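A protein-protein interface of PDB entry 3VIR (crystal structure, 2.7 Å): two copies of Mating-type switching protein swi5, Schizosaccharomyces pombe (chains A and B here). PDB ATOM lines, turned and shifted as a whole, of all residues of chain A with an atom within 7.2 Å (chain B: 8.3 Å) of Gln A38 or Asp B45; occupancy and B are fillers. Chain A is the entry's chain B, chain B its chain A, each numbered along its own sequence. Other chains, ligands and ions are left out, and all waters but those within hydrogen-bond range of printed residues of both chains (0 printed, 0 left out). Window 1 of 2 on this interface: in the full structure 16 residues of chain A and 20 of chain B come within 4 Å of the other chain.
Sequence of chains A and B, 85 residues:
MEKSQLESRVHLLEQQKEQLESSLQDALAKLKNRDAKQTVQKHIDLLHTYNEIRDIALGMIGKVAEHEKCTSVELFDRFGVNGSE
OD1 of Asp A45 lies within hydrogen-bond range of NE2 of Gln B38 (2.8 Å). NE2 of Gln A38 sits at hydrogen-bond distance from OD1 of Asp B45 (2.8 Å). The side-chain carboxylate of Glu B52 lies within salt-bridge range of the guanidinium group of Arg A34.
The side-chain amide nitrogen (NE2) of Gln B41 is in hydrogen-bond range of the side-chain carboxylate (OD2) of Asp B45. O of Asp B45 is in hydrogen-bond range of OG1 of Thr B49, 3.3 Å away. The side-chain amide nitrogen (NE2) of Gln A41 lies within hydrogen-bond range of the side-chain carboxylate (OD2) of Asp A45 (3.0 Å).
Among the printed residues, pairs that only touch across the chains: Lys A42 with Gln B38 (3.1 Å), Arg A34 with Asp B45 (3.4 Å), Arg A34 with His B48 (3.6 Å) and Arg A34 with Thr B49 (3.9 Å).
Of chain B, only Asp B45 (2.8 Å) comes within 4 Å of Gln A38. Asp B45 touches two residues of chain A. Of the printed residues of chain A, Glu B52 touches Arg A34 (3.1 Å). Printed residues of chain A within 4 Å of Thr B49: Arg A34 (3.9 Å). Of the printed residues of chain A, His B48 touches Arg A34 (3.6 Å). Printed residues of chain B within 4 Å of Arg A34: Asp B45 (3.4 Å), His B48 (3.6 Å), Thr B49 (3.9 Å) and Glu B52 (3.1 Å). Of the printed residues of chain B, Asp A45 touches Gln B38 (2.8 Å). Asn A33 touches none of the printed residues of chain B. The nearest residue of chain B that does not touch Gln A38 is Lys B42 (4.1 Å).
Along chain B the printed residues that touch a printed residue of chain A span positions 38 to 52. Among the printed residues, 7 pairs touch across the chains.
Gln A38 touches Asp B45, and with the chains exchanged Asp A45 touches Gln B38. Lys A42 touches Gln B38, but with the chains exchanged Gln A38 does not touch Lys B42 (4.1 Å). Positions printed for both chains: 38, 39, 40, 41, 42, 43, 44 and 45. Of the 7 pairs that touch across the chains among the printed residues, 2 have their exchanged pair printed and touching as well.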
ATOM      1  N   LEU A  31     -34.006 -21.290 -13.982  1.00  0.00           N
ATOM      2  CA  LEU A  31     -33.134 -22.185 -14.723  1.00  0.00           C
ATOM      3  C   LEU A  31     -33.404 -22.003 -16.187  1.00  0.00           C
ATOM      4  O   LEU A  31     -32.585 -21.427 -16.894  1.00  0.00           O
ATOM      5  CB  LEU A  31     -33.412 -23.636 -14.342  1.00  0.00           C
ATOM      6  CG  LEU A  31     -32.591 -24.693 -15.061  1.00  0.00           C
ATOM      7  CD1 LEU A  31     -33.099 -26.102 -14.752  1.00  0.00           C
ATOM      8  CD2 LEU A  31     -32.557 -24.418 -16.584  1.00  0.00           C
ATOM      9  N   LYS A  32     -34.574 -22.443 -16.659  1.00  0.00           N
ATOM     10  CA  LYS A  32     -34.853 -22.443 -18.090  1.00  0.00           C
ATOM     11  C   LYS A  32     -34.378 -21.128 -18.729  1.00  0.00           C
ATOM     12  O   LYS A  32     -33.915 -21.107 -19.846  1.00  0.00           O
ATOM     13  CB  LYS A  32     -36.339 -22.696 -18.362  1.00  0.00           C
ATOM     14  CG  LYS A  32     -36.755 -24.220 -18.304  1.00  0.00           C
ATOM     15  CD  LYS A  32     -38.164 -24.496 -18.988  1.00  0.00           C
ATOM     16  CE  LYS A  32     -39.010 -25.573 -18.245  1.00  0.00           C
ATOM     17  NZ  LYS A  32     -39.997 -25.063 -17.147  1.00  0.00           N
ATOM     18  N   ASN A  33     -34.466 -20.038 -17.997  1.00  0.00           N
ATOM     19  CA  ASN A  33     -34.228 -18.734 -18.541  1.00  0.00           C
ATOM     20  C   ASN A  33     -32.760 -18.584 -18.820  1.00  0.00           C
ATOM     21  O   ASN A  33     -32.319 -18.123 -19.907  1.00  0.00           O
ATOM     22  CB  ASN A  33     -34.626 -17.725 -17.479  1.00  0.00           C
ATOM     23  CG  ASN A  33     -34.420 -16.311 -17.906  1.00  0.00           C
ATOM     24  OD1 ASN A  33     -33.301 -15.865 -18.135  1.00  0.00           O
ATOM     25  ND2 ASN A  33     -35.505 -15.574 -17.974  1.00  0.00           N
ATOM     26  N   ARG A  34     -31.979 -18.964 -17.822  1.00  0.00           N
ATOM     27  CA  ARG A  34     -30.592 -18.711 -17.907  1.00  0.00           C
ATOM     28  C   ARG A  34     -29.986 -19.738 -18.841  1.00  0.00           C
ATOM     29  O   ARG A  34     -28.913 -19.502 -19.415  1.00  0.00           O
ATOM     30  CB  ARG A  34     -29.983 -18.684 -16.527  1.00  0.00           C
ATOM     31  CG  ARG A  34     -29.703 -19.982 -15.952  1.00  0.00           C
ATOM     32  CD  ARG A  34     -29.064 -19.818 -14.626  1.00  0.00           C
ATOM     33  NE  ARG A  34     -29.721 -20.677 -13.668  1.00  0.00           N
ATOM     34  CZ  ARG A  34     -30.294 -20.234 -12.562  1.00  0.00           C
ATOM     35  NH1 ARG A  34     -30.265 -18.928 -12.257  1.00  0.00           N
ATOM     36  NH2 ARG A  34     -30.831 -21.103 -11.738  1.00  0.00           N
ATOM     37  N   ASP A  35     -30.696 -20.843 -19.027  1.00  0.00           N
ATOM     38  CA  ASP A  35     -30.421 -21.795 -20.123  1.00  0.00           C
ATOM     39  C   ASP A  35     -30.623 -21.259 -21.545  1.00  0.00           C
ATOM     40  O   ASP A  35     -29.952 -21.638 -22.488  1.00  0.00           O
ATOM     41  CB  ASP A  35     -31.395 -22.941 -19.985  1.00  0.00           C
ATOM     42  CG  ASP A  35     -30.827 -24.230 -20.447  1.00  0.00           C
ATOM     43  OD1 ASP A  35     -30.590 -24.343 -21.687  1.00  0.00           O
ATOM     44  OD2 ASP A  35     -30.642 -25.107 -19.540  1.00  0.00           O
ATOM     45  N   ALA A  36     -31.639 -20.433 -21.689  1.00  0.00           N
ATOM     46  CA  ALA A  36     -32.002 -19.847 -22.949  1.00  0.00           C
ATOM     47  C   ALA A  36     -30.901 -18.886 -23.247  1.00  0.00           C
ATOM     48  O   ALA A  36     -30.263 -18.981 -24.288  1.00  0.00           O
ATOM     49  CB  ALA A  36     -33.341 -19.119 -22.823  1.00  0.00           C
ATOM     50  N   LYS A  37     -30.661 -17.993 -22.286  1.00  0.00           N
ATOM     51  CA  LYS A  37     -29.661 -16.908 -22.406  1.00  0.00           C
ATOM     52  C   LYS A  37     -28.296 -17.434 -22.894  1.00  0.00           C
ATOM     53  O   LYS A  37     -27.584 -16.781 -23.676  1.00  0.00           O
ATOM     54  CB  LYS A  37     -29.523 -16.194 -21.057  1.00  0.00           C
ATOM     55  CG  LYS A  37     -29.134 -14.757 -21.146  1.00  0.00           C
ATOM     56  CD  LYS A  37     -29.379 -13.995 -19.826  1.00  0.00           C
ATOM     57  CE  LYS A  37     -30.873 -13.777 -19.523  1.00  0.00           C
ATOM     58  NZ  LYS A  37     -31.169 -12.518 -18.745  1.00  0.00           N
ATOM     59  N   GLN A  38     -27.979 -18.650 -22.455  1.00  0.00           N
ATOM     60  CA  GLN A  38     -26.742 -19.310 -22.811  1.00  0.00           C
ATOM     61  C   GLN A  38     -26.821 -19.836 -24.230  1.00  0.00           C
ATOM     62  O   GLN A  38     -25.908 -19.605 -25.011  1.00  0.00           O
ATOM     63  CB  GLN A  38     -26.330 -20.303 -21.691  1.00  0.00           C
ATOM     64  CG  GLN A  38     -26.073 -21.800 -21.960  1.00  0.00           C
ATOM     65  CD  GLN A  38     -25.834 -22.593 -20.601  1.00  0.00           C
ATOM     66  OE1 GLN A  38     -25.890 -23.830 -20.559  1.00  0.00           O
ATOM     67  NE2 GLN A  38     -25.579 -21.859 -19.511  1.00  0.00           N
ATOM     68  N   THR A  39     -27.930 -20.426 -24.626  1.00  0.00           N
ATOM     69  CA  THR A  39     -28.125 -20.748 -26.059  1.00  0.00           C
ATOM     70  C   THR A  39     -28.115 -19.537 -27.039  1.00  0.00           C
ATOM     71  O   THR A  39     -27.621 -19.641 -28.167  1.00  0.00           O
ATOM     72  CB  THR A  39     -29.393 -21.567 -26.294  1.00  0.00           C
ATOM     73  OG1 THR A  39     -29.016 -22.926 -26.504  1.00  0.00           O
ATOM     74  CG2 THR A  39     -30.085 -21.103 -27.523  1.00  0.00           C
ATOM     75  N   VAL A  40     -28.657 -18.394 -26.632  1.00  0.00           N
ATOM     76  CA  VAL A  40     -28.599 -17.221 -27.498  1.00  0.00           C
ATOM     77  C   VAL A  40     -27.103 -16.960 -27.661  1.00  0.00           C
ATOM     78  O   VAL A  40     -26.587 -16.765 -28.769  1.00  0.00           O
ATOM     79  CB  VAL A  40     -29.344 -16.015 -26.871  1.00  0.00           C
ATOM     80  CG1 VAL A  40     -29.001 -14.725 -27.561  1.00  0.00           C
ATOM     81  CG2 VAL A  40     -30.842 -16.249 -26.927  1.00  0.00           C
ATOM     82  N   GLN A  41     -26.391 -17.028 -26.544  1.00  0.00           N
ATOM     83  CA  GLN A  41     -24.978 -16.740 -26.549  1.00  0.00           C
ATOM     84  C   GLN A  41     -24.128 -17.702 -27.385  1.00  0.00           C
ATOM     85  O   GLN A  41     -23.160 -17.273 -28.032  1.00  0.00           O
ATOM     86  CB  GLN A  41     -24.466 -16.755 -25.147  1.00  0.00           C
ATOM     87  CG  GLN A  41     -23.087 -16.237 -25.052  1.00  0.00           C
ATOM     88  CD  GLN A  41     -23.010 -14.797 -25.408  1.00  0.00           C
ATOM     89  OE1 GLN A  41     -23.707 -13.961 -24.791  1.00  0.00           O
ATOM     90  NE2 GLN A  41     -22.168 -14.471 -26.395  1.00  0.00           N
ATOM     91  N   LYS A  42     -24.436 -18.993 -27.370  1.00  0.00           N
ATOM     92  CA  LYS A  42     -23.700 -19.862 -28.269  1.00  0.00           C
ATOM     93  C   LYS A  42     -23.890 -19.300 -29.689  1.00  0.00           C
ATOM     94  O   LYS A  42     -22.938 -19.093 -30.429  1.00  0.00           O
ATOM     95  CB  LYS A  42     -24.107 -21.343 -28.126  1.00  0.00           C
ATOM     96  CG  LYS A  42     -23.278 -22.114 -27.055  1.00  0.00           C
ATOM     97  CD  LYS A  42     -24.075 -23.209 -26.253  1.00  0.00           C
ATOM     98  CE  LYS A  42     -23.662 -24.684 -26.588  1.00  0.00           C
ATOM     99  NZ  LYS A  42     -22.215 -25.026 -26.343  1.00  0.00           N
ATOM    100  N   HIS A  43     -25.118 -18.961 -30.036  1.00  0.00           N
ATOM    101  CA  HIS A  43     -25.415 -18.562 -31.400  1.00  0.00           C
ATOM    102  C   HIS A  43     -24.696 -17.280 -31.856  1.00  0.00           C
ATOM    103  O   HIS A  43     -24.045 -17.273 -32.913  1.00  0.00           O
ATOM    104  CB  HIS A  43     -26.919 -18.505 -31.597  1.00  0.00           C
ATOM    105  CG  HIS A  43     -27.542 -19.854 -31.704  1.00  0.00           C
ATOM    106  ND1 HIS A  43     -27.303 -20.691 -32.774  1.00  0.00           N
ATOM    107  CD2 HIS A  43     -28.377 -20.525 -30.882  1.00  0.00           C
ATOM    108  CE1 HIS A  43     -27.983 -21.811 -32.613  1.00  0.00           C
ATOM    109  NE2 HIS A  43     -28.641 -21.737 -31.473  1.00  0.00           N
ATOM    110  N   ILE A  44     -24.770 -16.234 -31.042  1.00  0.00           N
ATOM    111  CA  ILE A  44     -24.060 -14.982 -31.308  1.00  0.00           C
ATOM    112  C   ILE A  44     -22.515 -15.168 -31.429  1.00  0.00           C
ATOM    113  O   ILE A  44     -21.855 -14.562 -32.272  1.00  0.00           O
ATOM    114  CB  ILE A  44     -24.283 -13.994 -30.154  1.00  0.00           C
ATOM    115  CG1 ILE A  44     -25.763 -13.660 -29.998  1.00  0.00           C
ATOM    116  CG2 ILE A  44     -23.489 -12.749 -30.380  1.00  0.00           C
ATOM    117  CD1 ILE A  44     -26.139 -13.105 -28.666  1.00  0.00           C
ATOM    118  N   ASP A  45     -21.933 -15.985 -30.560  1.00  0.00           N
ATOM    119  CA  ASP A  45     -20.498 -16.250 -30.609  1.00  0.00           C
ATOM    120  C   ASP A  45     -20.112 -16.982 -31.882  1.00  0.00           C
ATOM    121  O   ASP A  45     -19.024 -16.769 -32.449  1.00  0.00           O
ATOM    122  CB  ASP A  45     -20.070 -17.092 -29.403  1.00  0.00           C
ATOM    123  CG  ASP A  45     -19.939 -16.267 -28.123  1.00  0.00           C
ATOM    124  OD1 ASP A  45     -19.872 -16.889 -27.033  1.00  0.00           O
ATOM    125  OD2 ASP A  45     -19.872 -15.009 -28.224  1.00  0.00           O
ATOM    126  N   GLN B  38     -17.931 -18.737 -21.871  1.00  0.00           N
ATOM    127  CA  GLN B  38     -19.202 -19.415 -21.807  1.00  0.00           C
ATOM    128  C   GLN B  38     -19.041 -20.762 -21.089  1.00  0.00           C
ATOM    129  O   GLN B  38     -20.031 -21.367 -20.698  1.00  0.00           O
ATOM    130  CB  GLN B  38     -19.841 -19.519 -23.225  1.00  0.00           C
ATOM    131  CG  GLN B  38     -19.473 -20.774 -24.043  1.00  0.00           C
ATOM    132  CD  GLN B  38     -19.984 -20.762 -25.516  1.00  0.00           C
ATOM    133  OE1 GLN B  38     -20.404 -21.810 -26.038  1.00  0.00           O
ATOM    134  NE2 GLN B  38     -19.917 -19.600 -26.187  1.00  0.00           N
ATOM    135  N   THR B  39     -17.822 -21.248 -20.880  1.00  0.00           N
ATOM    136  CA  THR B  39     -17.670 -22.372 -19.937  1.00  0.00           C
ATOM    137  C   THR B  39     -17.813 -21.900 -18.495  1.00  0.00           C
ATOM    138  O   THR B  39     -18.567 -22.487 -17.723  1.00  0.00           O
ATOM    139  CB  THR B  39     -16.366 -23.152 -20.119  1.00  0.00           C
ATOM    140  OG1 THR B  39     -16.481 -23.945 -21.305  1.00  0.00           O
ATOM    141  CG2 THR B  39     -16.123 -24.081 -18.934  1.00  0.00           C
ATOM    142  N   VAL B  40     -17.124 -20.829 -18.112  1.00  0.00           N
ATOM    143  CA  VAL B  40     -17.283 -20.362 -16.726  1.00  0.00           C
ATOM    144  C   VAL B  40     -18.762 -20.095 -16.500  1.00  0.00           C
ATOM    145  O   VAL B  40     -19.267 -20.312 -15.400  1.00  0.00           O
ATOM    146  CB  VAL B  40     -16.428 -19.120 -16.342  1.00  0.00           C
ATOM    147  CG1 VAL B  40     -15.072 -19.150 -17.061  1.00  0.00           C
ATOM    148  CG2 VAL B  40     -17.169 -17.839 -16.636  1.00  0.00           C
ATOM    149  N   GLN B  41     -19.466 -19.683 -17.555  1.00  0.00           N
ATOM    150  CA  GLN B  41     -20.902 -19.429 -17.437  1.00  0.00           C
ATOM    151  C   GLN B  41     -21.772 -20.666 -17.270  1.00  0.00           C
ATOM    152  O   GLN B  41     -22.809 -20.599 -16.621  1.00  0.00           O
ATOM    153  CB  GLN B  41     -21.427 -18.654 -18.618  1.00  0.00           C
ATOM    154  CG  GLN B  41     -22.838 -18.170 -18.392  1.00  0.00           C
ATOM    155  CD  GLN B  41     -22.891 -17.004 -17.443  1.00  0.00           C
ATOM    156  OE1 GLN B  41     -22.316 -15.949 -17.725  1.00  0.00           O
ATOM    157  NE2 GLN B  41     -23.584 -17.174 -16.311  1.00  0.00           N
ATOM    158  N   LYS B  42     -21.388 -21.774 -17.884  1.00  0.00           N
ATOM    159  CA  LYS B  42     -22.078 -23.026 -17.650  1.00  0.00           C
ATOM    160  C   LYS B  42     -21.954 -23.337 -16.177  1.00  0.00           C
ATOM    161  O   LYS B  42     -22.933 -23.655 -15.525  1.00  0.00           O
ATOM    162  CB  LYS B  42     -21.466 -24.171 -18.459  1.00  0.00           C
ATOM    163  CG  LYS B  42     -21.878 -24.226 -19.930  1.00  0.00           C
ATOM    164  CD  LYS B  42     -21.759 -25.671 -20.482  1.00  0.00           C
ATOM    165  CE  LYS B  42     -21.082 -25.734 -21.862  1.00  0.00           C
ATOM    166  NZ  LYS B  42     -20.490 -27.083 -22.089  1.00  0.00           N
ATOM    167  N   HIS B  43     -20.735 -23.213 -15.660  1.00  0.00           N
ATOM    168  CA  HIS B  43     -20.426 -23.546 -14.274  1.00  0.00           C
ATOM    169  C   HIS B  43     -21.137 -22.666 -13.285  1.00  0.00           C
ATOM    170  O   HIS B  43     -21.724 -23.172 -12.368  1.00  0.00           O
ATOM    171  CB  HIS B  43     -18.928 -23.461 -14.035  1.00  0.00           C
ATOM    172  CG  HIS B  43     -18.174 -24.630 -14.574  1.00  0.00           C
ATOM    173  ND1 HIS B  43     -17.772 -24.712 -15.888  1.00  0.00           N
ATOM    174  CD2 HIS B  43     -17.755 -25.772 -13.980  1.00  0.00           C
ATOM    175  CE1 HIS B  43     -17.133 -25.854 -16.082  1.00  0.00           C
ATOM    176  NE2 HIS B  43     -17.106 -26.512 -14.938  1.00  0.00           N
ATOM    177  N   ILE B  44     -21.086 -21.354 -13.473  1.00  0.00           N
ATOM    178  CA  ILE B  44     -21.854 -20.431 -12.639  1.00  0.00           C
ATOM    179  C   ILE B  44     -23.390 -20.756 -12.613  1.00  0.00           C
ATOM    180  O   ILE B  44     -24.108 -20.516 -11.631  1.00  0.00           O
ATOM    181  CB  ILE B  44     -21.703 -19.002 -13.158  1.00  0.00           C
ATOM    182  CG1 ILE B  44     -20.266 -18.474 -12.972  1.00  0.00           C
ATOM    183  CG2 ILE B  44     -22.725 -18.087 -12.479  1.00  0.00           C
ATOM    184  CD1 ILE B  44     -19.673 -18.651 -11.551  1.00  0.00           C
ATOM    185  N   ASP B  45     -23.895 -21.285 -13.709  1.00  0.00           N
ATOM    186  CA  ASP B  45     -25.290 -21.587 -13.785  1.00  0.00           C
ATOM    187  C   ASP B  45     -25.573 -22.880 -13.058  1.00  0.00           C
ATOM    188  O   ASP B  45     -26.598 -22.996 -12.381  1.00  0.00           O
ATOM    189  CB  ASP B  45     -25.714 -21.726 -15.242  1.00  0.00           C
ATOM    190  CG  ASP B  45     -25.888 -20.379 -15.947  1.00  0.00           C
ATOM    191  OD1 ASP B  45     -26.177 -20.426 -17.170  1.00  0.00           O
ATOM    192  OD2 ASP B  45     -25.781 -19.308 -15.279  1.00  0.00           O
ATOM    193  N   LEU B  46     -24.698 -23.872 -13.205  1.00  0.00           N
ATOM    194  CA  LEU B  46     -24.880 -25.128 -12.483  1.00  0.00           C
ATOM    195  C   LEU B  46     -24.844 -24.850 -10.989  1.00  0.00           C
ATOM    196  O   LEU B  46     -25.586 -25.416 -10.201  1.00  0.00           O
ATOM    197  CB  LEU B  46     -23.804 -26.139 -12.859  1.00  0.00           C
ATOM    198  CG  LEU B  46     -24.177 -27.361 -13.714  1.00  0.00           C
ATOM    199  CD1 LEU B  46     -25.479 -27.187 -14.534  1.00  0.00           C
ATOM    200  CD2 LEU B  46     -23.002 -27.758 -14.631  1.00  0.00           C
ATOM    201  N   LEU B  47     -23.995 -23.934 -10.597  1.00  0.00           N
ATOM    202  CA  LEU B  47     -23.924 -23.607  -9.206  1.00  0.00           C
ATOM    203  C   LEU B  47     -25.239 -22.952  -8.774  1.00  0.00           C
ATOM    204  O   LEU B  47     -25.713 -23.190  -7.680  1.00  0.00           O
ATOM    205  CB  LEU B  47     -22.706 -22.694  -8.924  1.00  0.00           C
ATOM    206  CG  LEU B  47     -22.043 -22.707  -7.527  1.00  0.00           C
ATOM    207  CD1 LEU B  47     -21.951 -24.080  -6.786  1.00  0.00           C
ATOM    208  CD2 LEU B  47     -20.657 -22.099  -7.757  1.00  0.00           C
ATOM    209  N   HIS B  48     -25.814 -22.106  -9.611  1.00  0.00           N
ATOM    210  CA  HIS B  48     -27.064 -21.478  -9.237  1.00  0.00           C
ATOM    211  C   HIS B  48     -28.189 -22.550  -9.001  1.00  0.00           C
ATOM    212  O   HIS B  48     -28.906 -22.515  -7.985  1.00  0.00           O
ATOM    213  CB  HIS B  48     -27.463 -20.471 -10.308  1.00  0.00           C
ATOM    214  CG  HIS B  48     -26.916 -19.088 -10.102  1.00  0.00           C
ATOM    215  ND1 HIS B  48     -27.170 -18.342  -8.970  1.00  0.00           N
ATOM    216  CD2 HIS B  48     -26.183 -18.290 -10.915  1.00  0.00           C
ATOM    217  CE1 HIS B  48     -26.605 -17.153  -9.084  1.00  0.00           C
ATOM    218  NE2 HIS B  48     -25.995 -17.100 -10.255  1.00  0.00           N
ATOM    219  N   THR B  49     -28.300 -23.502  -9.931  1.00  0.00           N
ATOM    220  CA  THR B  49     -29.297 -24.575  -9.880  1.00  0.00           C
ATOM    221  C   THR B  49     -29.119 -25.475  -8.679  1.00  0.00           C
ATOM    222  O   THR B  49     -30.101 -25.951  -8.103  1.00  0.00           O
ATOM    223  CB  THR B  49     -29.193 -25.496 -11.125  1.00  0.00           C
ATOM    224  OG1 THR B  49     -29.363 -24.719 -12.320  1.00  0.00           O
ATOM    225  CG2 THR B  49     -30.251 -26.621 -11.072  1.00  0.00           C
ATOM    226  N   TYR B  50     -27.863 -25.759  -8.338  1.00  0.00           N
ATOM    227  CA  TYR B  50     -27.567 -26.638  -7.222  1.00  0.00           C
ATOM    228  C   TYR B  50     -27.937 -25.921  -5.936  1.00  0.00           C
ATOM    229  O   TYR B  50     -28.482 -26.517  -5.017  1.00  0.00           O
ATOM    230  CB  TYR B  50     -26.100 -27.028  -7.185  1.00  0.00           C
ATOM    231  CG  TYR B  50     -25.660 -27.480  -5.788  1.00  0.00           C
ATOM    232  CD1 TYR B  50     -25.193 -26.554  -4.829  1.00  0.00           C
ATOM    233  CD2 TYR B  50     -25.741 -28.837  -5.413  1.00  0.00           C
ATOM    234  CE1 TYR B  50     -24.812 -26.985  -3.537  1.00  0.00           C
ATOM    235  CE2 TYR B  50     -25.363 -29.271  -4.127  1.00  0.00           C
ATOM    236  CZ  TYR B  50     -24.904 -28.344  -3.206  1.00  0.00           C
ATOM    237  OH  TYR B  50     -24.521 -28.794  -1.970  1.00  0.00           O
ATOM    238  N   ASN B  51     -27.657 -24.636  -5.846  1.00  0.00           N
ATOM    239  CA  ASN B  51     -28.012 -23.968  -4.624  1.00  0.00           C
ATOM    240  C   ASN B  51     -29.499 -24.004  -4.427  1.00  0.00           C
ATOM    241  O   ASN B  51     -29.933 -24.162  -3.284  1.00  0.00           O
ATOM    242  CB  ASN B  51     -27.483 -22.537  -4.531  1.00  0.00           C
ATOM    243  CG  ASN B  51     -26.012 -22.497  -4.168  1.00  0.00           C
ATOM    244  OD1 ASN B  51     -25.167 -22.794  -5.010  1.00  0.00           O
ATOM    245  ND2 ASN B  51     -25.697 -22.156  -2.917  1.00  0.00           N
ATOM    246  N   GLU B  52     -30.263 -23.894  -5.523  1.00  0.00           N
ATOM    247  CA  GLU B  52     -31.725 -23.764  -5.428  1.00  0.00           C
ATOM    248  C   GLU B  52     -32.362 -25.105  -5.077  1.00  0.00           C
ATOM    249  O   GLU B  52     -33.182 -25.188  -4.168  1.00  0.00           O
ATOM    250  CB  GLU B  52     -32.346 -23.179  -6.721  1.00  0.00           C
ATOM    251  CG  GLU B  52     -32.402 -21.598  -6.832  1.00  0.00           C
ATOM    252  CD  GLU B  52     -32.283 -21.035  -8.300  1.00  0.00           C
ATOM    253  OE1 GLU B  52     -32.610 -21.768  -9.289  1.00  0.00           O
ATOM    254  OE2 GLU B  52     -31.855 -19.852  -8.455  1.00  0.00           O
